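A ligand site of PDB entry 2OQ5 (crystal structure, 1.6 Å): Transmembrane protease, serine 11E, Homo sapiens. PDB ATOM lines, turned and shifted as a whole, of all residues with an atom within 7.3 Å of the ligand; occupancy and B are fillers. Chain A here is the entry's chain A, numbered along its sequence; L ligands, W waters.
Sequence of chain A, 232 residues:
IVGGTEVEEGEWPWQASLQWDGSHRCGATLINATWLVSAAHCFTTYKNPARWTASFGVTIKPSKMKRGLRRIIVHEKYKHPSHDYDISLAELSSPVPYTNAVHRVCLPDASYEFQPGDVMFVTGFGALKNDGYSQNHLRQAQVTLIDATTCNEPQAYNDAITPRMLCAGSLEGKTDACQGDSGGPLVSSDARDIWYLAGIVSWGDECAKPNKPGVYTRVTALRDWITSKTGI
A nitrogen (N1) of the ligand lies within hydrogen-bond range of the backbone carbonyl oxygen (O) of Glu 206, 2.8 Å away.
A nitrogen (N1) of the ligand is in salt-bridge range of the side-chain carboxylate (OD2) of Asp 176, 2.8 Å away.
O of Ala 177 lies close to N2 of the ligand, 3.3 Å away.
The backbone NH (N) of Ala 208 sits at hydrogen-bond distance from the side-chain carboxylate (OD2) of Asp 176, at 2.9 Å.
OG of Ser 182 sits close to NE2 of His 41, 3.1 Å away.
O of Ala 168 is in hydrogen-bond range of N of Gly 214 (3.1 Å).
SG of Cys 207 sits at hydrogen-bond distance from NE2 of Gln 179 (3.3 Å).
The backbone NH (N) of Val 215 lies within hydrogen-bond range of the backbone carbonyl oxygen (O) of Trp 203.
SG of Cys 207 is disulfide-bonded to SG of Cys 178.
The backbone NH (N) of Cys 207 is in hydrogen-bond range of the side-chain amide oxygen (OD1) of Asn 130, 2.7 Å away.
The side-chain carboxylate (OD2) of Asp 181 sits at hydrogen-bond distance from the backbone NH (N) of Cys 178.
Residues that only touch the ligand: Cys 178, Gln 179, Ser 182, Val 201, Ser 202, Trp 203, Gly 204, Cys 207 and Gly 214.
Hydrophobic or aromatic side chains within 4 Å of the ligand: Ala 177 and Val 201.
12 residues have an atom within 4 Å of the ligand: Asp 176, Ala 177, Cys 178, Gln 179, Ser 182, Val 201, Ser 202, Trp 203, Gly 204, Glu 206, Cys 207 and Gly 214.
Along chain A the residues within 4 Å of the ligand span positions 176 to 214.
Water W1 lies within hydrogen-bond range of the backbone carbonyl oxygen (O) of Val 215, a nitrogen (N2) of the ligand and the backbone carbonyl oxygen (O) of Trp 203.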
ATOM      1  N   HIS A  41     -24.951  -7.105  14.784  1.00  0.00           N
ATOM      2  CA  HIS A  41     -26.152  -6.344  15.108  1.00  0.00           C
ATOM      3  C   HIS A  41     -27.467  -7.086  14.866  1.00  0.00           C
ATOM      4  O   HIS A  41     -28.501  -6.695  15.401  1.00  0.00           O
ATOM      5  CB  HIS A  41     -26.151  -4.945  14.455  1.00  0.00           C
ATOM      6  CG  HIS A  41     -26.526  -4.938  13.011  1.00  0.00           C
ATOM      7  ND1 HIS A  41     -25.589  -4.803  11.998  1.00  0.00           N
ATOM      8  CD2 HIS A  41     -27.740  -4.984  12.394  1.00  0.00           C
ATOM      9  CE1 HIS A  41     -26.208  -4.763  10.835  1.00  0.00           C
ATOM     10  NE2 HIS A  41     -27.510  -4.868  11.044  1.00  0.00           N
ATOM     11  N   ASN A 130     -35.797   3.328   1.675  1.00  0.00           N
ATOM     12  CA  ASN A 130     -35.698   3.650   3.095  1.00  0.00           C
ATOM     13  C   ASN A 130     -37.046   3.380   3.753  1.00  0.00           C
ATOM     14  O   ASN A 130     -38.087   3.768   3.225  1.00  0.00           O
ATOM     15  CB  ASN A 130     -35.371   5.136   3.286  1.00  0.00           C
ATOM     16  CG  ASN A 130     -34.034   5.523   2.682  1.00  0.00           C
ATOM     17  OD1 ASN A 130     -33.009   4.919   2.981  1.00  0.00           O
ATOM     18  ND2 ASN A 130     -34.041   6.545   1.833  1.00  0.00           N
ATOM     19  N   TYR A 157     -18.187   9.840   5.459  1.00  0.00           N
ATOM     20  CA  TYR A 157     -18.318   9.364   6.826  1.00  0.00           C
ATOM     21  C   TYR A 157     -17.426  10.030   7.863  1.00  0.00           C
ATOM     22  O   TYR A 157     -17.405   9.616   9.031  1.00  0.00           O
ATOM     23  CB  TYR A 157     -18.244   7.842   6.876  1.00  0.00           C
ATOM     24  CG  TYR A 157     -19.475   7.211   6.263  1.00  0.00           C
ATOM     25  CD1 TYR A 157     -19.411   6.564   5.033  1.00  0.00           C
ATOM     26  CD2 TYR A 157     -20.715   7.314   6.894  1.00  0.00           C
ATOM     27  CE1 TYR A 157     -20.569   6.054   4.430  1.00  0.00           C
ATOM     28  CE2 TYR A 157     -21.870   6.805   6.305  1.00  0.00           C
ATOM     29  CZ  TYR A 157     -21.784   6.180   5.077  1.00  0.00           C
ATOM     30  OH  TYR A 157     -22.928   5.667   4.507  1.00  0.00           O
ATOM     31  N   ALA A 168     -18.497   0.286  -0.159  1.00  0.00           N
ATOM     32  CA  ALA A 168     -18.835  -0.137  -1.504  1.00  0.00           C
ATOM     33  C   ALA A 168     -20.200   0.398  -1.898  1.00  0.00           C
ATOM     34  O   ALA A 168     -21.096   0.526  -1.055  1.00  0.00           O
ATOM     35  CB  ALA A 168     -18.815  -1.663  -1.623  1.00  0.00           C
ATOM     36  N   ASP A 176     -27.401   0.183  -3.714  1.00  0.00           N
ATOM     37  CA  ASP A 176     -26.944   0.067  -2.328  1.00  0.00           C
ATOM     38  C   ASP A 176     -27.757  -1.000  -1.612  1.00  0.00           C
ATOM     39  O   ASP A 176     -28.809  -1.448  -2.103  1.00  0.00           O
ATOM     40  CB  ASP A 176     -27.152   1.420  -1.614  1.00  0.00           C
ATOM     41  CG  ASP A 176     -26.469   1.500  -0.241  1.00  0.00           C
ATOM     42  OD1 ASP A 176     -25.622   0.642   0.095  1.00  0.00           O
ATOM     43  OD2 ASP A 176     -26.777   2.465   0.497  1.00  0.00           O
ATOM     44  N   ALA A 177     -27.222  -1.482  -0.502  1.00  0.00           N
ATOM     45  CA  ALA A 177     -27.931  -2.450   0.334  1.00  0.00           C
ATOM     46  C   ALA A 177     -28.828  -1.563   1.201  1.00  0.00           C
ATOM     47  O   ALA A 177     -28.660  -0.344   1.241  1.00  0.00           O
ATOM     48  CB  ALA A 177     -26.951  -3.228   1.205  1.00  0.00           C
ATOM     49  N   CYS A 178     -29.782  -2.167   1.895  1.00  0.00           N
ATOM     50  CA  CYS A 178     -30.698  -1.408   2.745  1.00  0.00           C
ATOM     51  C   CYS A 178     -31.133  -2.260   3.934  1.00  0.00           C
ATOM     52  O   CYS A 178     -30.610  -3.353   4.119  1.00  0.00           O
ATOM     53  CB  CYS A 178     -31.910  -0.947   1.910  1.00  0.00           C
ATOM     54  SG  CYS A 178     -32.838   0.459   2.596  1.00  0.00           S
ATOM     55  N   GLN A 179     -32.052  -1.756   4.754  1.00  0.00           N
ATOM     56  CA  GLN A 179     -32.528  -2.496   5.925  1.00  0.00           C
ATOM     57  C   GLN A 179     -33.057  -3.861   5.487  1.00  0.00           C
ATOM     58  O   GLN A 179     -33.778  -3.960   4.496  1.00  0.00           O
ATOM     59  CB  GLN A 179     -33.631  -1.721   6.662  1.00  0.00           C
ATOM     60  CG  GLN A 179     -33.159  -0.440   7.354  1.00  0.00           C
ATOM     61  CD  GLN A 179     -33.229   0.794   6.471  1.00  0.00           C
ATOM     62  OE1 GLN A 179     -34.290   1.123   5.933  1.00  0.00           O
ATOM     63  NE2 GLN A 179     -32.108   1.486   6.325  1.00  0.00           N
ATOM     64  N   GLY A 180     -32.682  -4.903   6.221  1.00  0.00           N
ATOM     65  CA  GLY A 180     -33.110  -6.242   5.859  1.00  0.00           C
ATOM     66  C   GLY A 180     -32.029  -6.987   5.099  1.00  0.00           C
ATOM     67  O   GLY A 180     -32.079  -8.212   4.977  1.00  0.00           O
ATOM     68  N   ASP A 181     -31.067  -6.242   4.542  1.00  0.00           N
ATOM     69  CA  ASP A 181     -29.962  -6.857   3.812  1.00  0.00           C
ATOM     70  C   ASP A 181     -28.812  -7.107   4.780  1.00  0.00           C
ATOM     71  O   ASP A 181     -27.898  -7.861   4.464  1.00  0.00           O
ATOM     72  CB  ASP A 181     -29.465  -5.951   2.680  1.00  0.00           C
ATOM     73  CG  ASP A 181     -30.466  -5.838   1.557  1.00  0.00           C
ATOM     74  OD1 ASP A 181     -31.003  -6.875   1.137  1.00  0.00           O
ATOM     75  OD2 ASP A 181     -30.700  -4.711   1.087  1.00  0.00           O
ATOM     76  N   SER A 182     -28.864  -6.452   5.941  1.00  0.00           N
ATOM     77  CA  SER A 182     -27.844  -6.565   6.979  1.00  0.00           C
ATOM     78  C   SER A 182     -27.425  -8.004   7.240  1.00  0.00           C
ATOM     79  O   SER A 182     -28.265  -8.886   7.343  1.00  0.00           O
ATOM     80  CB  SER A 182     -28.360  -5.960   8.295  1.00  0.00           C
ATOM     81  OG  SER A 182     -28.607  -4.576   8.143  1.00  0.00           O
ATOM     82  N   GLY A 183     -26.116  -8.219   7.321  1.00  0.00           N
ATOM     83  CA  GLY A 183     -25.579  -9.550   7.574  1.00  0.00           C
ATOM     84  C   GLY A 183     -25.341 -10.363   6.321  1.00  0.00           C
ATOM     85  O   GLY A 183     -24.721 -11.434   6.379  1.00  0.00           O
ATOM     86  N   VAL A 201     -22.804  -7.031   4.872  1.00  0.00           N
ATOM     87  CA  VAL A 201     -23.638  -5.826   4.949  1.00  0.00           C
ATOM     88  C   VAL A 201     -23.746  -5.400   6.401  1.00  0.00           C
ATOM     89  O   VAL A 201     -24.217  -6.163   7.250  1.00  0.00           O
ATOM     90  CB  VAL A 201     -25.036  -6.057   4.350  1.00  0.00           C
ATOM     91  CG1 VAL A 201     -25.865  -4.786   4.427  1.00  0.00           C
ATOM     92  CG2 VAL A 201     -24.919  -6.532   2.910  1.00  0.00           C
ATOM     93  N   SER A 202     -23.322  -4.169   6.698  1.00  0.00           N
ATOM     94  CA  SER A 202     -23.316  -3.679   8.062  1.00  0.00           C
ATOM     95  C   SER A 202     -24.168  -2.437   8.342  1.00  0.00           C
ATOM     96  O   SER A 202     -25.135  -2.511   9.100  1.00  0.00           O
ATOM     97  CB  SER A 202     -21.869  -3.427   8.510  1.00  0.00           C
ATOM     98  OG  SER A 202     -21.796  -3.053   9.872  1.00  0.00           O
ATOM     99  N   TRP A 203     -23.798  -1.297   7.754  1.00  0.00           N
ATOM    100  CA  TRP A 203     -24.554  -0.069   7.980  1.00  0.00           C
ATOM    101  C   TRP A 203     -24.406   0.960   6.872  1.00  0.00           C
ATOM    102  O   TRP A 203     -23.765   0.704   5.846  1.00  0.00           O
ATOM    103  CB  TRP A 203     -24.175   0.551   9.337  1.00  0.00           C
ATOM    104  CG  TRP A 203     -22.735   0.981   9.459  1.00  0.00           C
ATOM    105  CD1 TRP A 203     -21.634   0.172   9.569  1.00  0.00           C
ATOM    106  CD2 TRP A 203     -22.243   2.336   9.512  1.00  0.00           C
ATOM    107  NE1 TRP A 203     -20.491   0.932   9.681  1.00  0.00           N
ATOM    108  CE2 TRP A 203     -20.833   2.257   9.647  1.00  0.00           C
ATOM    109  CE3 TRP A 203     -22.854   3.596   9.453  1.00  0.00           C
ATOM    110  CZ2 TRP A 203     -20.032   3.414   9.723  1.00  0.00           C
ATOM    111  CZ3 TRP A 203     -22.054   4.732   9.536  1.00  0.00           C
ATOM    112  CH2 TRP A 203     -20.650   4.632   9.665  1.00  0.00           C
ATOM    113  N   GLY A 204     -25.032   2.105   7.079  1.00  0.00           N
ATOM    114  CA  GLY A 204     -24.981   3.194   6.112  1.00  0.00           C
ATOM    115  C   GLY A 204     -25.889   4.318   6.567  1.00  0.00           C
ATOM    116  O   GLY A 204     -26.612   4.177   7.547  1.00  0.00           O
ATOM    117  N   ASP A 205     -25.778   5.462   5.906  1.00  0.00           N
ATOM    118  CA  ASP A 205     -26.626   6.604   6.228  1.00  0.00           C
ATOM    119  C   ASP A 205     -27.849   6.409   5.322  1.00  0.00           C
ATOM    120  O   ASP A 205     -27.774   6.698   4.121  1.00  0.00           O
ATOM    121  CB  ASP A 205     -25.908   7.912   5.902  1.00  0.00           C
ATOM    122  CG  ASP A 205     -26.667   9.141   6.377  1.00  0.00           C
ATOM    123  OD1 ASP A 205     -27.864   9.032   6.712  1.00  0.00           O
ATOM    124  OD2 ASP A 205     -26.056  10.235   6.406  1.00  0.00           O
ATOM    125  N   GLU A 206     -28.934   5.906   5.897  1.00  0.00           N
ATOM    126  CA  GLU A 206     -30.157   5.616   5.136  1.00  0.00           C
ATOM    127  C   GLU A 206     -29.805   4.592   4.051  1.00  0.00           C
ATOM    128  O   GLU A 206     -29.058   3.652   4.310  1.00  0.00           O
ATOM    129  CB  GLU A 206     -30.769   6.896   4.544  1.00  0.00           C
ATOM    130  CG  GLU A 206     -31.181   7.927   5.608  1.00  0.00           C
ATOM    131  CD  GLU A 206     -32.212   8.918   5.101  1.00  0.00           C
ATOM    132  OE1 GLU A 206     -31.938   9.645   4.121  1.00  0.00           O
ATOM    133  OE2 GLU A 206     -33.315   8.975   5.690  1.00  0.00           O
ATOM    134  N   CYS A 207     -30.331   4.770   2.843  1.00  0.00           N
ATOM    135  CA  CYS A 207     -30.049   3.850   1.739  1.00  0.00           C
ATOM    136  C   CYS A 207     -29.948   4.589   0.416  1.00  0.00           C
ATOM    137  O   CYS A 207     -30.792   5.426   0.101  1.00  0.00           O
ATOM    138  CB  CYS A 207     -31.146   2.779   1.623  1.00  0.00           C
ATOM    139  SG  CYS A 207     -31.414   1.799   3.126  1.00  0.00           S
ATOM    140  N   ALA A 208     -28.920   4.263  -0.351  1.00  0.00           N
ATOM    141  CA  ALA A 208     -28.681   4.860  -1.666  1.00  0.00           C
ATOM    142  C   ALA A 208     -28.574   6.382  -1.660  1.00  0.00           C
ATOM    143  O   ALA A 208     -29.002   7.046  -2.600  1.00  0.00           O
ATOM    144  CB  ALA A 208     -29.767   4.398  -2.645  1.00  0.00           C
ATOM    145  N   LYS A 209     -28.012   6.922  -0.584  1.00  0.00           N
ATOM    146  CA  LYS A 209     -27.829   8.362  -0.459  1.00  0.00           C
ATOM    147  C   LYS A 209     -26.527   8.796  -1.112  1.00  0.00           C
ATOM    148  O   LYS A 209     -25.500   8.135  -0.967  1.00  0.00           O
ATOM    149  CB  LYS A 209     -27.818   8.797   1.014  1.00  0.00           C
ATOM    150  CG  LYS A 209     -29.204   8.984   1.610  1.00  0.00           C
ATOM    151  CD  LYS A 209     -29.297  10.303   2.360  1.00  0.00           C
ATOM    152  CE  LYS A 209     -28.349  10.363   3.540  1.00  0.00           C
ATOM    153  NZ  LYS A 209     -28.461  11.648   4.295  1.00  0.00           N
ATOM    154  N   LYS A 212     -22.791   8.859   0.473  1.00  0.00           N
ATOM    155  CA  LYS A 212     -22.851   7.960   1.632  1.00  0.00           C
ATOM    156  C   LYS A 212     -22.966   6.517   1.161  1.00  0.00           C
ATOM    157  O   LYS A 212     -24.047   5.918   1.217  1.00  0.00           O
ATOM    158  CB  LYS A 212     -24.050   8.318   2.538  1.00  0.00           C
ATOM    159  CG  LYS A 212     -24.050   9.744   3.089  1.00  0.00           C
ATOM    160  CD  LYS A 212     -22.797  10.026   3.916  1.00  0.00           C
ATOM    161  CE  LYS A 212     -22.774  11.467   4.424  1.00  0.00           C
ATOM    162  NZ  LYS A 212     -23.751  11.708   5.514  1.00  0.00           N
ATOM    163  N   PRO A 213     -21.851   5.923   0.714  1.00  0.00           N
ATOM    164  CA  PRO A 213     -21.872   4.531   0.234  1.00  0.00           C
ATOM    165  C   PRO A 213     -22.150   3.541   1.368  1.00  0.00           C
ATOM    166  O   PRO A 213     -22.063   3.893   2.543  1.00  0.00           O
ATOM    167  CB  PRO A 213     -20.468   4.348  -0.330  1.00  0.00           C
ATOM    168  CG  PRO A 213     -19.638   5.222   0.555  1.00  0.00           C
ATOM    169  CD  PRO A 213     -20.478   6.469   0.671  1.00  0.00           C
ATOM    170  N   GLY A 214     -22.497   2.316   1.001  1.00  0.00           N
ATOM    171  CA  GLY A 214     -22.754   1.299   2.013  1.00  0.00           C
ATOM    172  C   GLY A 214     -21.489   0.912   2.761  1.00  0.00           C
ATOM    173  O   GLY A 214     -20.400   0.910   2.191  1.00  0.00           O
ATOM    174  N   VAL A 215     -21.637   0.629   4.053  1.00  0.00           N
ATOM    175  CA  VAL A 215     -20.490   0.220   4.847  1.00  0.00           C
ATOM    176  C   VAL A 215     -20.628  -1.254   5.163  1.00  0.00           C
ATOM    177  O   VAL A 215     -21.719  -1.742   5.491  1.00  0.00           O
ATOM    178  CB  VAL A 215     -20.322   1.058   6.127  1.00  0.00           C
ATOM    179  CG1 VAL A 215     -19.020   0.701   6.822  1.00  0.00           C
ATOM    180  CG2 VAL A 215     -20.316   2.527   5.757  1.00  0.00           C
ATOM    181  N   TYR A 216     -19.517  -1.967   5.001  1.00  0.00           N
ATOM    182  CA  TYR A 216     -19.493  -3.407   5.195  1.00  0.00           C
ATOM    183  C   TYR A 216     -18.387  -3.829   6.152  1.00  0.00           C
ATOM    184  O   TYR A 216     -17.361  -3.167   6.256  1.00  0.00           O
ATOM    185  CB  TYR A 216     -19.239  -4.093   3.851  1.00  0.00           C
ATOM    186  CG  TYR A 216     -20.286  -3.830   2.798  1.00  0.00           C
ATOM    187  CD1 TYR A 216     -20.353  -2.602   2.133  1.00  0.00           C
ATOM    188  CD2 TYR A 216     -21.213  -4.816   2.471  1.00  0.00           C
ATOM    189  CE1 TYR A 216     -21.336  -2.364   1.158  1.00  0.00           C
ATOM    190  CE2 TYR A 216     -22.184  -4.593   1.508  1.00  0.00           C
ATOM    191  CZ  TYR A 216     -22.244  -3.369   0.848  1.00  0.00           C
ATOM    192  OH  TYR A 216     -23.222  -3.164  -0.098  1.00  0.00           O
HETATM  193  C1  LIG L   1     -27.376   0.030   4.811  1.00  0.00           C
HETATM  194  C2  LIG L   1     -27.023  -1.290   5.170  1.00  0.00           C
HETATM  195  C3  LIG L   1     -27.608  -1.922   6.289  1.00  0.00           C
HETATM  196  C4  LIG L   1     -28.568  -1.252   7.069  1.00  0.00           C
HETATM  197  C5  LIG L   1     -28.942   0.070   6.723  1.00  0.00           C
HETATM  198  C6  LIG L   1     -28.349   0.698   5.609  1.00  0.00           C
HETATM  199  C7  LIG L   1     -26.778   0.664   3.675  1.00  0.00           C
HETATM  200  N1  LIG L   1     -27.142   1.891   3.253  1.00  0.00           N
HETATM  201  N2  LIG L   1     -25.818   0.079   2.932  1.00  0.00           N
HETATM  202  O   HOH W   1     -23.882  -1.994   3.621  1.00  0.00           O
HETATM  203  O   HOH W   2     -27.548   1.730   9.407  1.00  0.00           O
